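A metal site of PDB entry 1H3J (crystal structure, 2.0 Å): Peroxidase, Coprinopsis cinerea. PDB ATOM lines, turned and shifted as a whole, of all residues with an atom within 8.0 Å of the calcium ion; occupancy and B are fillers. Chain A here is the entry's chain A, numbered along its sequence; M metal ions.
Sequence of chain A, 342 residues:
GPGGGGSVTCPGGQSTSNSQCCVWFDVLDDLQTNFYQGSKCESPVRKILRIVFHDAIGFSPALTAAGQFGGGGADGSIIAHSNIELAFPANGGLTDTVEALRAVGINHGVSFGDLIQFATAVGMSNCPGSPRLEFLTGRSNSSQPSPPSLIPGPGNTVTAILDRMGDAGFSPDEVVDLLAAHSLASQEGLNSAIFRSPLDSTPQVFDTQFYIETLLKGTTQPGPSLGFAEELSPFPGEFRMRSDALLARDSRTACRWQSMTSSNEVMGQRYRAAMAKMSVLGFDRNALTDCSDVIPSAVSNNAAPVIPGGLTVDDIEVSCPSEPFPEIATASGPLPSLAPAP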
ATOM      1  N   PRO A 128      16.835  -1.370  -4.547  1.00  0.00           N
ATOM      2  CA  PRO A 128      15.790  -1.647  -3.571  1.00  0.00           C
ATOM      3  C   PRO A 128      14.420  -1.363  -4.133  1.00  0.00           C
ATOM      4  O   PRO A 128      14.215  -0.362  -4.814  1.00  0.00           O
ATOM      5  CB  PRO A 128      16.093  -0.655  -2.444  1.00  0.00           C
ATOM      6  CG  PRO A 128      17.539  -0.535  -2.465  1.00  0.00           C
ATOM      7  CD  PRO A 128      17.861  -0.483  -3.967  1.00  0.00           C
ATOM      8  N   ALA A 180       7.512   2.852 -15.481  1.00  0.00           N
ATOM      9  CA  ALA A 180       7.940   2.795 -14.068  1.00  0.00           C
ATOM     10  C   ALA A 180       9.474   2.809 -14.062  1.00  0.00           C
ATOM     11  O   ALA A 180      10.111   3.221 -13.063  1.00  0.00           O
ATOM     12  CB  ALA A 180       7.369   1.523 -13.358  1.00  0.00           C
ATOM     13  N   ALA A 181      10.083   2.420 -15.196  1.00  0.00           N
ATOM     14  CA  ALA A 181      11.538   2.429 -15.296  1.00  0.00           C
ATOM     15  C   ALA A 181      12.151   3.818 -15.074  1.00  0.00           C
ATOM     16  O   ALA A 181      13.322   3.945 -14.733  1.00  0.00           O
ATOM     17  CB  ALA A 181      12.001   1.856 -16.661  1.00  0.00           C
ATOM     18  N   HIS A 182      11.362   4.878 -15.287  1.00  0.00           N
ATOM     19  CA  HIS A 182      11.853   6.247 -15.066  1.00  0.00           C
ATOM     20  C   HIS A 182      11.983   6.567 -13.569  1.00  0.00           C
ATOM     21  O   HIS A 182      12.395   7.651 -13.187  1.00  0.00           O
ATOM     22  CB  HIS A 182      10.956   7.291 -15.766  1.00  0.00           C
ATOM     23  CG  HIS A 182      11.280   7.432 -17.245  1.00  0.00           C
ATOM     24  ND1 HIS A 182      10.720   8.390 -18.038  1.00  0.00           N
ATOM     25  CD2 HIS A 182      12.167   6.669 -18.007  1.00  0.00           C
ATOM     26  CE1 HIS A 182      11.241   8.188 -19.243  1.00  0.00           C
ATOM     27  NE2 HIS A 182      12.073   7.187 -19.309  1.00  0.00           N
ATOM     28  N   SER A 183      11.565   5.623 -12.728  1.00  0.00           N
ATOM     29  CA  SER A 183      11.743   5.764 -11.302  1.00  0.00           C
ATOM     30  C   SER A 183      13.219   5.509 -10.985  1.00  0.00           C
ATOM     31  O   SER A 183      13.662   5.736  -9.859  1.00  0.00           O
ATOM     32  CB  SER A 183      10.849   4.761 -10.588  1.00  0.00           C
ATOM     33  OG  SER A 183      10.970   4.886  -9.176  1.00  0.00           O
ATOM     34  N   LEU A 184      14.000   5.011 -11.957  1.00  0.00           N
ATOM     35  CA  LEU A 184      15.446   4.738 -11.792  1.00  0.00           C
ATOM     36  C   LEU A 184      16.076   5.415 -13.007  1.00  0.00           C
ATOM     37  O   LEU A 184      16.690   4.749 -13.849  1.00  0.00           O
ATOM     38  CB  LEU A 184      15.713   3.236 -11.900  1.00  0.00           C
ATOM     39  CG  LEU A 184      15.128   2.333 -10.784  1.00  0.00           C
ATOM     40  CD1 LEU A 184      15.169   0.901 -11.218  1.00  0.00           C
ATOM     41  CD2 LEU A 184      15.938   2.516  -9.497  1.00  0.00           C
ATOM     42  N   ALA A 185      15.971   6.738 -13.086  1.00  0.00           N
ATOM     43  CA  ALA A 185      16.421   7.455 -14.269  1.00  0.00           C
ATOM     44  C   ALA A 185      16.926   8.856 -14.056  1.00  0.00           C
ATOM     45  O   ALA A 185      16.504   9.561 -13.125  1.00  0.00           O
ATOM     46  CB  ALA A 185      15.264   7.516 -15.256  1.00  0.00           C
ATOM     47  N   PRO A 198      18.152  13.598 -11.942  1.00  0.00           N
ATOM     48  CA  PRO A 198      17.167  12.511 -11.874  1.00  0.00           C
ATOM     49  C   PRO A 198      15.763  12.905 -12.254  1.00  0.00           C
ATOM     50  O   PRO A 198      15.362  14.071 -12.129  1.00  0.00           O
ATOM     51  CB  PRO A 198      17.216  12.110 -10.396  1.00  0.00           C
ATOM     52  CG  PRO A 198      18.536  12.633  -9.896  1.00  0.00           C
ATOM     53  CD  PRO A 198      18.630  13.954 -10.594  1.00  0.00           C
ATOM     54  N   LEU A 199      14.986  11.897 -12.628  1.00  0.00           N
ATOM     55  CA  LEU A 199      13.611  12.081 -13.017  1.00  0.00           C
ATOM     56  C   LEU A 199      12.695  11.987 -11.782  1.00  0.00           C
ATOM     57  O   LEU A 199      11.491  12.252 -11.880  1.00  0.00           O
ATOM     58  CB  LEU A 199      13.220  11.067 -14.110  1.00  0.00           C
ATOM     59  CG  LEU A 199      13.478  11.422 -15.607  1.00  0.00           C
ATOM     60  CD1 LEU A 199      14.706  12.263 -15.819  1.00  0.00           C
ATOM     61  CD2 LEU A 199      13.509  10.183 -16.470  1.00  0.00           C
ATOM     62  N   ASP A 200      13.231  11.505 -10.662  1.00  0.00           N
ATOM     63  CA  ASP A 200      12.457  11.455  -9.405  1.00  0.00           C
ATOM     64  C   ASP A 200      13.416  11.625  -8.228  1.00  0.00           C
ATOM     65  O   ASP A 200      14.630  11.627  -8.424  1.00  0.00           O
ATOM     66  CB  ASP A 200      11.430  10.299  -9.302  1.00  0.00           C
ATOM     67  CG  ASP A 200      12.031   8.948  -8.828  1.00  0.00           C
ATOM     68  OD1 ASP A 200      13.245   8.785  -8.630  1.00  0.00           O
ATOM     69  OD2 ASP A 200      11.205   8.043  -8.660  1.00  0.00           O
ATOM     70  N   SER A 201      12.889  11.848  -7.022  1.00  0.00           N
ATOM     71  CA  SER A 201      13.777  12.077  -5.884  1.00  0.00           C
ATOM     72  C   SER A 201      14.595  10.864  -5.407  1.00  0.00           C
ATOM     73  O   SER A 201      15.538  11.022  -4.617  1.00  0.00           O
ATOM     74  CB  SER A 201      13.004  12.711  -4.712  1.00  0.00           C
ATOM     75  OG  SER A 201      11.827  11.957  -4.424  1.00  0.00           O
ATOM     76  N   THR A 202      14.266   9.686  -5.927  1.00  0.00           N
ATOM     77  CA  THR A 202      14.932   8.423  -5.554  1.00  0.00           C
ATOM     78  C   THR A 202      15.330   7.628  -6.799  1.00  0.00           C
ATOM     79  O   THR A 202      14.630   6.646  -7.167  1.00  0.00           O
ATOM     80  CB  THR A 202      13.958   7.563  -4.766  1.00  0.00           C
ATOM     81  OG1 THR A 202      12.750   7.401  -5.514  1.00  0.00           O
ATOM     82  CG2 THR A 202      13.590   8.233  -3.416  1.00  0.00           C
ATOM     83  N   PRO A 203      16.391   8.078  -7.520  1.00  0.00           N
ATOM     84  CA  PRO A 203      16.894   7.429  -8.749  1.00  0.00           C
ATOM     85  C   PRO A 203      17.527   6.071  -8.476  1.00  0.00           C
ATOM     86  O   PRO A 203      17.868   5.366  -9.426  1.00  0.00           O
ATOM     87  CB  PRO A 203      17.925   8.418  -9.273  1.00  0.00           C
ATOM     88  CG  PRO A 203      18.446   9.077  -8.005  1.00  0.00           C
ATOM     89  CD  PRO A 203      17.174   9.301  -7.238  1.00  0.00           C
ATOM     90  N   GLN A 204      17.726   5.728  -7.194  1.00  0.00           N
ATOM     91  CA  GLN A 204      18.272   4.420  -6.801  1.00  0.00           C
ATOM     92  C   GLN A 204      17.204   3.545  -6.087  1.00  0.00           C
ATOM     93  O   GLN A 204      17.520   2.504  -5.508  1.00  0.00           O
ATOM     94  CB  GLN A 204      19.526   4.550  -5.944  1.00  0.00           C
ATOM     95  CG  GLN A 204      20.709   5.105  -6.674  1.00  0.00           C
ATOM     96  CD  GLN A 204      21.983   5.037  -5.845  1.00  0.00           C
ATOM     97  OE1 GLN A 204      22.135   5.804  -4.889  1.00  0.00           O
ATOM     98  NE2 GLN A 204      22.894   4.128  -6.202  1.00  0.00           N
ATOM     99  N   VAL A 205      15.933   3.953  -6.163  1.00  0.00           N
ATOM    100  CA  VAL A 205      14.874   3.177  -5.552  1.00  0.00           C
ATOM    101  C   VAL A 205      13.708   2.988  -6.524  1.00  0.00           C
ATOM    102  O   VAL A 205      13.085   3.963  -6.961  1.00  0.00           O
ATOM    103  CB  VAL A 205      14.354   3.841  -4.232  1.00  0.00           C
ATOM    104  CG1 VAL A 205      13.325   2.913  -3.573  1.00  0.00           C
ATOM    105  CG2 VAL A 205      15.511   4.112  -3.273  1.00  0.00           C
ATOM    106  N   PHE A 206      13.357   1.741  -6.797  1.00  0.00           N
ATOM    107  CA  PHE A 206      12.269   1.483  -7.703  1.00  0.00           C
ATOM    108  C   PHE A 206      11.007   1.684  -6.868  1.00  0.00           C
ATOM    109  O   PHE A 206      10.520   0.781  -6.181  1.00  0.00           O
ATOM    110  CB  PHE A 206      12.397   0.073  -8.295  1.00  0.00           C
ATOM    111  CG  PHE A 206      11.377  -0.238  -9.370  1.00  0.00           C
ATOM    112  CD1 PHE A 206      11.547   0.220 -10.678  1.00  0.00           C
ATOM    113  CD2 PHE A 206      10.238  -0.982  -9.073  1.00  0.00           C
ATOM    114  CE1 PHE A 206      10.604  -0.034 -11.656  1.00  0.00           C
ATOM    115  CE2 PHE A 206       9.270  -1.262 -10.050  1.00  0.00           C
ATOM    116  CZ  PHE A 206       9.451  -0.782 -11.340  1.00  0.00           C
ATOM    117  N   ASP A 207      10.468   2.887  -6.955  1.00  0.00           N
ATOM    118  CA  ASP A 207       9.276   3.287  -6.195  1.00  0.00           C
ATOM    119  C   ASP A 207       8.309   4.184  -6.998  1.00  0.00           C
ATOM    120  O   ASP A 207       8.626   4.623  -8.109  1.00  0.00           O
ATOM    121  CB  ASP A 207       9.713   3.990  -4.896  1.00  0.00           C
ATOM    122  CG  ASP A 207      10.582   5.204  -5.157  1.00  0.00           C
ATOM    123  OD1 ASP A 207      10.636   5.676  -6.320  1.00  0.00           O
ATOM    124  OD2 ASP A 207      11.191   5.708  -4.193  1.00  0.00           O
ATOM    125  N   THR A 208       7.145   4.468  -6.432  1.00  0.00           N
ATOM    126  CA  THR A 208       6.129   5.290  -7.088  1.00  0.00           C
ATOM    127  C   THR A 208       6.416   6.790  -7.140  1.00  0.00           C
ATOM    128  O   THR A 208       5.589   7.532  -7.650  1.00  0.00           O
ATOM    129  CB  THR A 208       4.763   5.098  -6.420  1.00  0.00           C
ATOM    130  OG1 THR A 208       4.827   5.590  -5.059  1.00  0.00           O
ATOM    131  CG2 THR A 208       4.358   3.632  -6.446  1.00  0.00           C
ATOM    132  N   GLN A 209       7.535   7.244  -6.572  1.00  0.00           N
ATOM    133  CA  GLN A 209       7.875   8.664  -6.574  1.00  0.00           C
ATOM    134  C   GLN A 209       7.760   9.365  -7.955  1.00  0.00           C
ATOM    135  O   GLN A 209       7.277  10.486  -8.047  1.00  0.00           O
ATOM    136  CB  GLN A 209       9.260   8.900  -5.972  1.00  0.00           C
ATOM    137  CG  GLN A 209       9.345   8.671  -4.446  1.00  0.00           C
ATOM    138  CD  GLN A 209       8.182   9.316  -3.646  1.00  0.00           C
ATOM    139  OE1 GLN A 209       7.486   8.621  -2.913  1.00  0.00           O
ATOM    140  NE2 GLN A 209       7.987  10.623  -3.775  1.00  0.00           N
ATOM    141  N   PHE A 210       8.168   8.669  -9.008  1.00  0.00           N
ATOM    142  CA  PHE A 210       8.109   9.189 -10.366  1.00  0.00           C
ATOM    143  C   PHE A 210       6.708   9.579 -10.754  1.00  0.00           C
ATOM    144  O   PHE A 210       6.499  10.636 -11.311  1.00  0.00           O
ATOM    145  CB  PHE A 210       8.668   8.139 -11.373  1.00  0.00           C
ATOM    146  CG  PHE A 210       8.416   8.476 -12.820  1.00  0.00           C
ATOM    147  CD1 PHE A 210       9.118   9.508 -13.446  1.00  0.00           C
ATOM    148  CD2 PHE A 210       7.466   7.755 -13.551  1.00  0.00           C
ATOM    149  CE1 PHE A 210       8.874   9.817 -14.811  1.00  0.00           C
ATOM    150  CE2 PHE A 210       7.213   8.046 -14.901  1.00  0.00           C
ATOM    151  CZ  PHE A 210       7.915   9.079 -15.527  1.00  0.00           C
ATOM    152  N   TYR A 211       5.745   8.715 -10.470  1.00  0.00           N
ATOM    153  CA  TYR A 211       4.364   9.003 -10.823  1.00  0.00           C
ATOM    154  C   TYR A 211       3.812  10.173 -10.019  1.00  0.00           C
ATOM    155  O   TYR A 211       3.058  11.001 -10.537  1.00  0.00           O
ATOM    156  CB  TYR A 211       3.495   7.750 -10.648  1.00  0.00           C
ATOM    157  CG  TYR A 211       3.879   6.630 -11.600  1.00  0.00           C
ATOM    158  CD1 TYR A 211       3.444   6.635 -12.927  1.00  0.00           C
ATOM    159  CD2 TYR A 211       4.677   5.570 -11.169  1.00  0.00           C
ATOM    160  CE1 TYR A 211       3.774   5.604 -13.809  1.00  0.00           C
ATOM    161  CE2 TYR A 211       5.005   4.533 -12.038  1.00  0.00           C
ATOM    162  CZ  TYR A 211       4.552   4.552 -13.354  1.00  0.00           C
ATOM    163  OH  TYR A 211       4.822   3.477 -14.162  1.00  0.00           O
ATOM    164  N   GLU A 213       5.671  12.692  -8.370  1.00  0.00           N
ATOM    165  CA  GLU A 213       6.402  13.886  -8.697  1.00  0.00           C
ATOM    166  C   GLU A 213       6.140  14.525 -10.062  1.00  0.00           C
ATOM    167  O   GLU A 213       6.182  15.755 -10.154  1.00  0.00           O
ATOM    168  CB  GLU A 213       7.868  13.680  -8.391  1.00  0.00           C
ATOM    169  CG  GLU A 213       8.030  13.354  -6.935  1.00  0.00           C
ATOM    170  CD  GLU A 213       9.428  12.952  -6.521  1.00  0.00           C
ATOM    171  OE1 GLU A 213       9.562  12.443  -5.389  1.00  0.00           O
ATOM    172  OE2 GLU A 213      10.382  13.154  -7.263  1.00  0.00           O
ATOM    173  N   ASN A 264       3.658   0.755  -4.079  1.00  0.00           N
ATOM    174  CA  ASN A 264       4.839   0.265  -4.740  1.00  0.00           C
ATOM    175  C   ASN A 264       4.598  -1.167  -5.241  1.00  0.00           C
ATOM    176  O   ASN A 264       5.026  -1.548  -6.342  1.00  0.00           O
ATOM    177  CB  ASN A 264       6.011   0.279  -3.765  1.00  0.00           C
ATOM    178  CG  ASN A 264       6.523   1.662  -3.520  1.00  0.00           C
ATOM    179  OD1 ASN A 264       6.732   2.414  -4.463  1.00  0.00           O
ATOM    180  ND2 ASN A 264       6.727   2.001  -2.253  1.00  0.00           N
ATOM    181  N   MET A 267       2.663  -1.264  -8.432  1.00  0.00           N
ATOM    182  CA  MET A 267       3.471  -0.731  -9.515  1.00  0.00           C
ATOM    183  C   MET A 267       4.350  -1.867 -10.044  1.00  0.00           C
ATOM    184  O   MET A 267       4.339  -2.175 -11.264  1.00  0.00           O
ATOM    185  CB  MET A 267       4.344   0.422  -9.003  1.00  0.00           C
ATOM    186  CG  MET A 267       5.142   1.102 -10.125  1.00  0.00           C
ATOM    187  SD  MET A 267       6.309   2.253  -9.506  1.00  0.00           S
ATOM    188  CE  MET A 267       7.328   1.217  -8.539  1.00  0.00           C
ATOM    189  N   ASN A 301      11.912  -2.128  -0.209  1.00  0.00           N
ATOM    190  CA  ASN A 301      11.871  -0.696   0.054  1.00  0.00           C
ATOM    191  C   ASN A 301      10.756  -0.575   1.076  1.00  0.00           C
ATOM    192  O   ASN A 301       9.622  -0.968   0.796  1.00  0.00           O
ATOM    193  CB  ASN A 301      11.484   0.076  -1.215  1.00  0.00           C
ATOM    194  CG  ASN A 301      11.099   1.544  -0.943  1.00  0.00           C
ATOM    195  OD1 ASN A 301      10.299   2.124  -1.675  1.00  0.00           O
ATOM    196  ND2 ASN A 301      11.732   2.151   0.069  1.00  0.00           N
HETATM  197 CA    CA M   1      12.709   6.197  -7.699  1.00  0.00          CA
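N of Gln 209 sits close to OD1 of Asp 207, at 3.5 Å.
The side-chain carboxylate of Asp 200 lies close to the backbone NH of Phe 210.
The calcium ion is bound by O of Thr 202.
The calcium ion is bound by O of Val 205 (2.4 Å).
The backbone carbonyl oxygen (O) of Ser 183 binds the calcium ion (2.4 Å).
The calcium ion is bound by OG1 of Thr 202 (2.5 Å).
The side-chain carboxylate (OD1) of Asp 207 is bound to the calcium ion.
The calcium ion is bound by OD2 of Asp 200 (2.6 Å).
The calcium ion is bound by the side-chain hydroxyl (OG) of Ser 183 (2.6 Å).
The calcium ion is bound by the side-chain carboxylate (OD1) of Asp 200 (2.8 Å).
Within 4 Å of the calcium ion: Ser 183, Asp 200, Thr 202, Val 205 and Asp 207.
The nearest printed residue that does not touch the calcium ion is Pro 203 (4.1 Å).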
